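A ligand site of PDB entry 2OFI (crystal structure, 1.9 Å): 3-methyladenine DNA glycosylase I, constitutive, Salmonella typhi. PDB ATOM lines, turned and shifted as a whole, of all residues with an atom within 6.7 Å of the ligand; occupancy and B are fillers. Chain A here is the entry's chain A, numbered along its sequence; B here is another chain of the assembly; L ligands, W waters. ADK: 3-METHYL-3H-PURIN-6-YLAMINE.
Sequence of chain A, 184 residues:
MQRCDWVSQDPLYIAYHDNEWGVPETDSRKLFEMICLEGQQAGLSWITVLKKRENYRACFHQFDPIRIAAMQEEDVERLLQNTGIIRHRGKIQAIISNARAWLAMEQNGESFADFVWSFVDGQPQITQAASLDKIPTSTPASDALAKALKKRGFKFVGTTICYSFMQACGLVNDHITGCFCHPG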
ATOM      1  N   TRP A   6      -2.474   5.896   5.379  1.00  0.00           N
ATOM      2  CA  TRP A   6      -3.093   5.735   6.684  1.00  0.00           C
ATOM      3  C   TRP A   6      -4.526   6.262   6.736  1.00  0.00           C
ATOM      4  O   TRP A   6      -5.223   6.099   7.736  1.00  0.00           O
ATOM      5  CB  TRP A   6      -2.223   6.388   7.750  1.00  0.00           C
ATOM      6  CG  TRP A   6      -1.746   7.792   7.380  1.00  0.00           C
ATOM      7  CD1 TRP A   6      -0.527   8.118   6.811  1.00  0.00           C
ATOM      8  CD2 TRP A   6      -2.443   9.024   7.540  1.00  0.00           C
ATOM      9  NE1 TRP A   6      -0.438   9.480   6.611  1.00  0.00           N
ATOM     10  CE2 TRP A   6      -1.618  10.059   7.026  1.00  0.00           C
ATOM     11  CE3 TRP A   6      -3.723   9.373   8.038  1.00  0.00           C
ATOM     12  CZ2 TRP A   6      -1.990  11.397   7.062  1.00  0.00           C
ATOM     13  CZ3 TRP A   6      -4.092  10.727   8.049  1.00  0.00           C
ATOM     14  CH2 TRP A   6      -3.238  11.708   7.543  1.00  0.00           C
ATOM     15  N   VAL A   7      -5.004   6.868   5.655  1.00  0.00           N
ATOM     16  CA  VAL A   7      -6.314   7.510   5.721  1.00  0.00           C
ATOM     17  C   VAL A   7      -7.331   6.398   5.521  1.00  0.00           C
ATOM     18  O   VAL A   7      -7.253   5.681   4.539  1.00  0.00           O
ATOM     19  CB  VAL A   7      -6.513   8.603   4.624  1.00  0.00           C
ATOM     20  CG1 VAL A   7      -7.871   9.346   4.821  1.00  0.00           C
ATOM     21  CG2 VAL A   7      -5.361   9.649   4.677  1.00  0.00           C
ATOM     22  N   TYR A  13     -11.910  11.356   9.098  1.00  0.00           N
ATOM     23  CA  TYR A  13     -10.461  11.149   8.947  1.00  0.00           C
ATOM     24  C   TYR A  13     -10.016  11.739   7.607  1.00  0.00           C
ATOM     25  O   TYR A  13      -8.938  12.355   7.475  1.00  0.00           O
ATOM     26  CB  TYR A  13     -10.171   9.634   8.947  1.00  0.00           C
ATOM     27  CG  TYR A  13      -8.811   9.273   9.486  1.00  0.00           C
ATOM     28  CD1 TYR A  13      -7.868  10.254   9.808  1.00  0.00           C
ATOM     29  CD2 TYR A  13      -8.474   7.925   9.723  1.00  0.00           C
ATOM     30  CE1 TYR A  13      -6.580   9.897  10.309  1.00  0.00           C
ATOM     31  CE2 TYR A  13      -7.218   7.570  10.245  1.00  0.00           C
ATOM     32  CZ  TYR A  13      -6.278   8.562  10.546  1.00  0.00           C
ATOM     33  OH  TYR A  13      -5.052   8.210  11.068  1.00  0.00           O
ATOM     34  N   TYR A  16      -9.803  15.624   7.950  1.00  0.00           N
ATOM     35  CA  TYR A  16      -8.617  15.919   8.763  1.00  0.00           C
ATOM     36  C   TYR A  16      -7.368  15.799   7.876  1.00  0.00           C
ATOM     37  O   TYR A  16      -6.528  16.706   7.838  1.00  0.00           O
ATOM     38  CB  TYR A  16      -8.553  14.909   9.950  1.00  0.00           C
ATOM     39  CG  TYR A  16      -7.247  15.024  10.694  1.00  0.00           C
ATOM     40  CD1 TYR A  16      -6.197  14.126  10.472  1.00  0.00           C
ATOM     41  CD2 TYR A  16      -7.049  16.103  11.552  1.00  0.00           C
ATOM     42  CE1 TYR A  16      -4.968  14.281  11.141  1.00  0.00           C
ATOM     43  CE2 TYR A  16      -5.835  16.270  12.234  1.00  0.00           C
ATOM     44  CZ  TYR A  16      -4.822  15.374  11.994  1.00  0.00           C
ATOM     45  OH  TYR A  16      -3.664  15.613  12.664  1.00  0.00           O
ATOM     46  N   TRP A  21      -3.898  17.990   8.242  1.00  0.00           N
ATOM     47  CA  TRP A  21      -2.652  17.304   8.475  1.00  0.00           C
ATOM     48  C   TRP A  21      -1.542  17.794   7.533  1.00  0.00           C
ATOM     49  O   TRP A  21      -1.765  17.835   6.317  1.00  0.00           O
ATOM     50  CB  TRP A  21      -2.846  15.809   8.282  1.00  0.00           C
ATOM     51  CG  TRP A  21      -1.703  14.948   8.785  1.00  0.00           C
ATOM     52  CD1 TRP A  21      -1.495  14.507  10.067  1.00  0.00           C
ATOM     53  CD2 TRP A  21      -0.695  14.363   7.970  1.00  0.00           C
ATOM     54  NE1 TRP A  21      -0.376  13.705  10.107  1.00  0.00           N
ATOM     55  CE2 TRP A  21       0.137  13.589   8.830  1.00  0.00           C
ATOM     56  CE3 TRP A  21      -0.364  14.448   6.579  1.00  0.00           C
ATOM     57  CZ2 TRP A  21       1.235  12.841   8.353  1.00  0.00           C
ATOM     58  CZ3 TRP A  21       0.721  13.680   6.098  1.00  0.00           C
ATOM     59  CH2 TRP A  21       1.511  12.887   7.009  1.00  0.00           C
ATOM     60  N   MET A  34      -2.524  20.388  19.727  1.00  0.00           N
ATOM     61  CA  MET A  34      -2.056  19.233  19.004  1.00  0.00           C
ATOM     62  C   MET A  34      -1.008  18.397  19.730  1.00  0.00           C
ATOM     63  O   MET A  34      -1.052  17.190  19.589  1.00  0.00           O
ATOM     64  CB  MET A  34      -1.615  19.623  17.578  1.00  0.00           C
ATOM     65  CG  MET A  34      -2.875  19.743  16.696  1.00  0.00           C
ATOM     66  SD  MET A  34      -3.861  17.969  16.329  1.00  0.00           S
ATOM     67  CE  MET A  34      -2.408  16.670  16.614  1.00  0.00           C
ATOM     68  N   GLU A  38      -1.752  14.437  20.506  1.00  0.00           N
ATOM     69  CA  GLU A  38      -0.775  13.372  20.133  1.00  0.00           C
ATOM     70  C   GLU A  38      -0.388  12.561  21.354  1.00  0.00           C
ATOM     71  O   GLU A  38      -0.249  11.351  21.265  1.00  0.00           O
ATOM     72  CB  GLU A  38       0.489  13.926  19.501  1.00  0.00           C
ATOM     73  CG  GLU A  38       0.249  14.616  18.159  1.00  0.00           C
ATOM     74  CD  GLU A  38      -0.230  13.650  17.042  1.00  0.00           C
ATOM     75  OE1 GLU A  38      -0.076  12.386  17.127  1.00  0.00           O
ATOM     76  OE2 GLU A  38      -0.748  14.186  16.050  1.00  0.00           O
ATOM     77  N   GLN A  41      -2.889   9.949  22.163  1.00  0.00           N
ATOM     78  CA  GLN A  41      -2.863   8.782  21.259  1.00  0.00           C
ATOM     79  C   GLN A  41      -1.972   7.635  21.746  1.00  0.00           C
ATOM     80  O   GLN A  41      -2.099   6.498  21.259  1.00  0.00           O
ATOM     81  CB  GLN A  41      -2.399   9.235  19.837  1.00  0.00           C
ATOM     82  CG  GLN A  41      -2.348   8.123  18.765  1.00  0.00           C
ATOM     83  CD  GLN A  41      -0.933   7.542  18.651  1.00  0.00           C
ATOM     84  OE1 GLN A  41       0.050   8.082  19.232  1.00  0.00           O
ATOM     85  NE2 GLN A  41      -0.817   6.443  17.930  1.00  0.00           N
ATOM     86  N   LEU A  44      -2.643   3.779  21.308  1.00  0.00           N
ATOM     87  CA  LEU A  44      -3.967   3.667  20.667  1.00  0.00           C
ATOM     88  C   LEU A  44      -3.824   4.091  19.216  1.00  0.00           C
ATOM     89  O   LEU A  44      -2.778   4.638  18.805  1.00  0.00           O
ATOM     90  CB  LEU A  44      -4.981   4.644  21.358  1.00  0.00           C
ATOM     91  CG  LEU A  44      -5.255   4.454  22.853  1.00  0.00           C
ATOM     92  CD1 LEU A  44      -6.276   5.483  23.302  1.00  0.00           C
ATOM     93  CD2 LEU A  44      -5.827   3.095  23.089  1.00  0.00           C
ATOM     94  N   SER A  45      -4.869   3.889  18.423  1.00  0.00           N
ATOM     95  CA  SER A  45      -4.889   4.497  17.067  1.00  0.00           C
ATOM     96  C   SER A  45      -5.251   5.962  17.091  1.00  0.00           C
ATOM     97  O   SER A  45      -6.063   6.424  17.917  1.00  0.00           O
ATOM     98  CB  SER A  45      -5.930   3.789  16.169  1.00  0.00           C
ATOM     99  OG  SER A  45      -7.216   3.863  16.744  1.00  0.00           O
ATOM    100  N   TRP A  46      -4.696   6.733  16.167  1.00  0.00           N
ATOM    101  CA  TRP A  46      -5.034   8.149  16.114  1.00  0.00           C
ATOM    102  C   TRP A  46      -6.537   8.388  15.893  1.00  0.00           C
ATOM    103  O   TRP A  46      -7.105   9.325  16.417  1.00  0.00           O
ATOM    104  CB  TRP A  46      -4.243   8.817  14.981  1.00  0.00           C
ATOM    105  CG  TRP A  46      -4.721  10.218  14.723  1.00  0.00           C
ATOM    106  CD1 TRP A  46      -5.380  10.648  13.606  1.00  0.00           C
ATOM    107  CD2 TRP A  46      -4.629  11.333  15.603  1.00  0.00           C
ATOM    108  NE1 TRP A  46      -5.654  11.995  13.723  1.00  0.00           N
ATOM    109  CE2 TRP A  46      -5.185  12.441  14.935  1.00  0.00           C
ATOM    110  CE3 TRP A  46      -4.052  11.521  16.880  1.00  0.00           C
ATOM    111  CZ2 TRP A  46      -5.267  13.721  15.498  1.00  0.00           C
ATOM    112  CZ3 TRP A  46      -4.119  12.809  17.458  1.00  0.00           C
ATOM    113  CH2 TRP A  46      -4.734  13.905  16.760  1.00  0.00           C
ATOM    114  N   ILE A  47      -7.192   7.569  15.065  1.00  0.00           N
ATOM    115  CA  ILE A  47      -8.618   7.802  14.806  1.00  0.00           C
ATOM    116  C   ILE A  47      -9.422   7.808  16.108  1.00  0.00           C
ATOM    117  O   ILE A  47     -10.424   8.529  16.221  1.00  0.00           O
ATOM    118  CB  ILE A  47      -9.192   6.756  13.757  1.00  0.00           C
ATOM    119  CG1 ILE A  47     -10.622   7.134  13.315  1.00  0.00           C
ATOM    120  CG2 ILE A  47      -9.136   5.327  14.302  1.00  0.00           C
ATOM    121  CD1 ILE A  47     -10.705   8.595  12.732  1.00  0.00           C
ATOM    122  N   LEU A 132       4.021   4.521   3.110  1.00  0.00           N
ATOM    123  CA  LEU A 132       4.115   4.773   4.542  1.00  0.00           C
ATOM    124  C   LEU A 132       5.316   4.082   5.169  1.00  0.00           C
ATOM    125  O   LEU A 132       5.938   4.608   6.076  1.00  0.00           O
ATOM    126  CB  LEU A 132       2.808   4.320   5.206  1.00  0.00           C
ATOM    127  CG  LEU A 132       2.665   4.529   6.710  1.00  0.00           C
ATOM    128  CD1 LEU A 132       2.800   6.015   7.098  1.00  0.00           C
ATOM    129  CD2 LEU A 132       1.308   3.948   7.079  1.00  0.00           C
ATOM    130  N   THR A 160       8.489   9.667  19.291  1.00  0.00           N
ATOM    131  CA  THR A 160       7.574   9.198  18.267  1.00  0.00           C
ATOM    132  C   THR A 160       6.332  10.105  18.288  1.00  0.00           C
ATOM    133  O   THR A 160       5.855  10.591  17.225  1.00  0.00           O
ATOM    134  CB  THR A 160       7.215   7.702  18.500  1.00  0.00           C
ATOM    135  OG1 THR A 160       8.412   6.929  18.388  1.00  0.00           O
ATOM    136  CG2 THR A 160       6.229   7.250  17.434  1.00  0.00           C
ATOM    137  N   ILE A 161       5.840  10.399  19.486  1.00  0.00           N
ATOM    138  CA  ILE A 161       4.748  11.383  19.635  1.00  0.00           C
ATOM    139  C   ILE A 161       5.163  12.721  19.008  1.00  0.00           C
ATOM    140  O   ILE A 161       4.370  13.364  18.283  1.00  0.00           O
ATOM    141  CB  ILE A 161       4.384  11.553  21.139  1.00  0.00           C
ATOM    142  CG1 ILE A 161       3.570  10.316  21.573  1.00  0.00           C
ATOM    143  CG2 ILE A 161       3.552  12.830  21.416  1.00  0.00           C
ATOM    144  CD1 ILE A 161       3.483  10.243  23.164  1.00  0.00           C
ATOM    145  N   SER A 164       5.077  12.570  15.191  1.00  0.00           N
ATOM    146  CA  SER A 164       3.690  12.633  14.707  1.00  0.00           C
ATOM    147  C   SER A 164       3.114  14.033  14.819  1.00  0.00           C
ATOM    148  O   SER A 164       2.389  14.484  13.927  1.00  0.00           O
ATOM    149  CB  SER A 164       2.790  11.647  15.467  1.00  0.00           C
ATOM    150  OG  SER A 164       3.281  10.343  15.125  1.00  0.00           O
ATOM    151  N   PHE A 165       3.427  14.722  15.921  1.00  0.00           N
ATOM    152  CA  PHE A 165       3.033  16.155  16.079  1.00  0.00           C
ATOM    153  C   PHE A 165       3.649  17.032  14.945  1.00  0.00           C
ATOM    154  O   PHE A 165       2.974  17.901  14.336  1.00  0.00           O
ATOM    155  CB  PHE A 165       3.524  16.615  17.442  1.00  0.00           C
ATOM    156  CG  PHE A 165       3.589  18.097  17.619  1.00  0.00           C
ATOM    157  CD1 PHE A 165       2.421  18.831  17.845  1.00  0.00           C
ATOM    158  CD2 PHE A 165       4.827  18.761  17.593  1.00  0.00           C
ATOM    159  CE1 PHE A 165       2.444  20.192  18.002  1.00  0.00           C
ATOM    160  CE2 PHE A 165       4.876  20.137  17.771  1.00  0.00           C
ATOM    161  CZ  PHE A 165       3.672  20.860  17.990  1.00  0.00           C
ATOM    162  N   GLN A 167       4.544  16.091  11.947  1.00  0.00           N
ATOM    163  CA  GLN A 167       3.831  15.809  10.713  1.00  0.00           C
ATOM    164  C   GLN A 167       2.515  16.524  10.737  1.00  0.00           C
ATOM    165  O   GLN A 167       2.125  17.167   9.758  1.00  0.00           O
ATOM    166  CB  GLN A 167       3.527  14.343  10.609  1.00  0.00           C
ATOM    167  CG  GLN A 167       4.831  13.504  10.404  1.00  0.00           C
ATOM    168  CD  GLN A 167       4.489  12.003  10.417  1.00  0.00           C
ATOM    169  OE1 GLN A 167       3.736  11.540  11.268  1.00  0.00           O
ATOM    170  NE2 GLN A 167       5.060  11.247   9.477  1.00  0.00           N
ATOM    171  N   ALA A 168       1.786  16.367  11.844  1.00  0.00           N
ATOM    172  CA  ALA A 168       0.410  16.860  11.881  1.00  0.00           C
ATOM    173  C   ALA A 168       0.344  18.359  11.695  1.00  0.00           C
ATOM    174  O   ALA A 168      -0.568  18.850  10.994  1.00  0.00           O
ATOM    175  CB  ALA A 168      -0.294  16.414  13.196  1.00  0.00           C
ATOM    176  O5' 3DR B   7       2.216  -0.582  17.128  1.00  0.00           O
ATOM    177  P   3DR B   7       2.072  -2.003  17.873  1.00  0.00           P
ATOM    178  OP1 3DR B   7       2.082  -3.260  16.914  1.00  0.00           O
ATOM    179  OP2 3DR B   7       3.109  -2.130  19.075  1.00  0.00           O
ATOM    180  C2' 3DR B   7      -0.058   2.865  18.960  1.00  0.00           C
ATOM    181  C5' 3DR B   7       2.368   0.590  17.945  1.00  0.00           C
ATOM    182  C4' 3DR B   7       1.551   1.810  17.473  1.00  0.00           C
ATOM    183  O4' 3DR B   7       0.231   1.389  17.104  1.00  0.00           O
ATOM    184  C1' 3DR B   7      -0.779   1.984  17.928  1.00  0.00           C
ATOM    185  C3' 3DR B   7       1.421   2.790  18.627  1.00  0.00           C
ATOM    186  O3' 3DR B   7       1.685   4.109  18.176  1.00  0.00           O
ATOM    187  P    DA B   8       3.087   4.789  17.829  1.00  0.00           P
ATOM    188  OP1  DA B   8       2.701   5.923  16.923  1.00  0.00           O
ATOM    189  OP2  DA B   8       4.085   3.785  17.342  1.00  0.00           O
ATOM    190  O5'  DA B   8       3.673   5.339  19.165  1.00  0.00           O
ATOM    191  C5'  DA B   8       2.951   6.414  19.843  1.00  0.00           C
ATOM    192  C4'  DA B   8       3.297   6.444  21.314  1.00  0.00           C
ATOM    193  O4'  DA B   8       2.718   5.241  21.905  1.00  0.00           O
ATOM    194  C3'  DA B   8       4.806   6.376  21.550  1.00  0.00           C
ATOM    195  O3'  DA B   8       5.136   7.238  22.587  1.00  0.00           O
ATOM    196  C2'  DA B   8       5.050   4.974  22.119  1.00  0.00           C
ATOM    197  C1'  DA B   8       3.684   4.711  22.775  1.00  0.00           C
ATOM    198  N9   DA B   8       3.383   3.298  23.060  1.00  0.00           N
ATOM    199  C8   DA B   8       3.889   2.168  22.481  1.00  0.00           C
ATOM    200  N7   DA B   8       3.422   1.076  23.057  1.00  0.00           N
ATOM    201  C5   DA B   8       2.599   1.514  24.073  1.00  0.00           C
ATOM    202  C6   DA B   8       1.851   0.839  25.063  1.00  0.00           C
ATOM    203  N6   DA B   8       1.806  -0.497  25.147  1.00  0.00           N
ATOM    204  N1   DA B   8       1.146   1.561  25.918  1.00  0.00           N
ATOM    205  C2   DA B   8       1.183   2.914  25.845  1.00  0.00           C
ATOM    206  N3   DA B   8       1.859   3.666  24.956  1.00  0.00           N
ATOM    207  C4   DA B   8       2.545   2.897  24.073  1.00  0.00           C
HETATM  208  N9  ADK L   1      -0.699   8.868  14.103  1.00  0.00           N
HETATM  209  C4  ADK L   1      -1.300   9.800  13.328  1.00  0.00           C
HETATM  210  N3  ADK L   1      -1.850   9.670  11.999  1.00  0.00           N
HETATM  211  C2  ADK L   1      -2.419  10.728  11.397  1.00  0.00           C
HETATM  212  N1  ADK L   1      -2.509  11.900  12.034  1.00  0.00           N
HETATM  213  C6  ADK L   1      -2.042  12.114  13.282  1.00  0.00           C
HETATM  214  N6  ADK L   1      -2.153  13.313  13.858  1.00  0.00           N
HETATM  215  C5  ADK L   1      -1.361  11.020  14.042  1.00  0.00           C
HETATM  216  N7  ADK L   1      -0.812  10.810  15.252  1.00  0.00           N
HETATM  217  C8  ADK L   1      -0.381   9.519  15.273  1.00  0.00           C
HETATM  218  C3A ADK L   1      -1.762   8.384  11.274  1.00  0.00           C
HETATM  219  O   HOH W   1       0.857  12.542  12.430  1.00  0.00           O
HETATM  220  O   HOH W   2       1.999   9.709  12.356  1.00  0.00           O
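N of Trp 21 sits at hydrogen-bond distance from O of Tyr 16, at 3.0 Å.
OG of Ser 164 lies within hydrogen-bond range of O of Thr 160, at 3.3 Å.
NE2 of Gln 41 is in hydrogen-bond range of O3' of 3DR 7 of chain B, at 3.4 Å.
The side-chain amide nitrogen (NE2) of Gln 41 sits at hydrogen-bond distance from the backbone carbonyl oxygen (O) of Leu 44.
Residues that only touch the ligand: Tyr 13 (3.3 Å), Trp 46 (3.3 Å), Ala 168 (3.7 Å), Ser 164 (3.7 Å), Trp 6 (3.7 Å) and Gln 41 (3.95 Å).
Hydrophobic or aromatic side chains that line the ligand: Trp 6, Tyr 16, Trp 21, Trp 46 and Ala 168.
Nine residues have an atom within 4 Å of the ligand: Trp 6, Tyr 13, Tyr 16, Trp 21, Glu 38, Gln 41, Trp 46, Ser 164 and Ala 168.
The nearest printed residue that does not touch the ligand is Met 34 (4.4 Å).
Water W1 lies within hydrogen-bond range of NE1 of Trp 21, O of Ser 164, OE1 of Gln 167 and N6 of the ligand.
Water W2 lies within hydrogen-bond range of the side-chain amide oxygen of Gln 167 (2.7 Å), the side-chain hydroxyl of Ser 164 (3.1 Å) and a nitrogen (N9) of the ligand (3.3 Å).
OE1 of Glu 38 lies within hydrogen-bond range of N7 of the ligand.
OH of Tyr 16 is in hydrogen-bond range of N6 of the ligand (3.0 Å).
A nitrogen (N1) of the ligand is in hydrogen-bond range of the indole nitrogen of Trp 21, 3.4 Å away.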
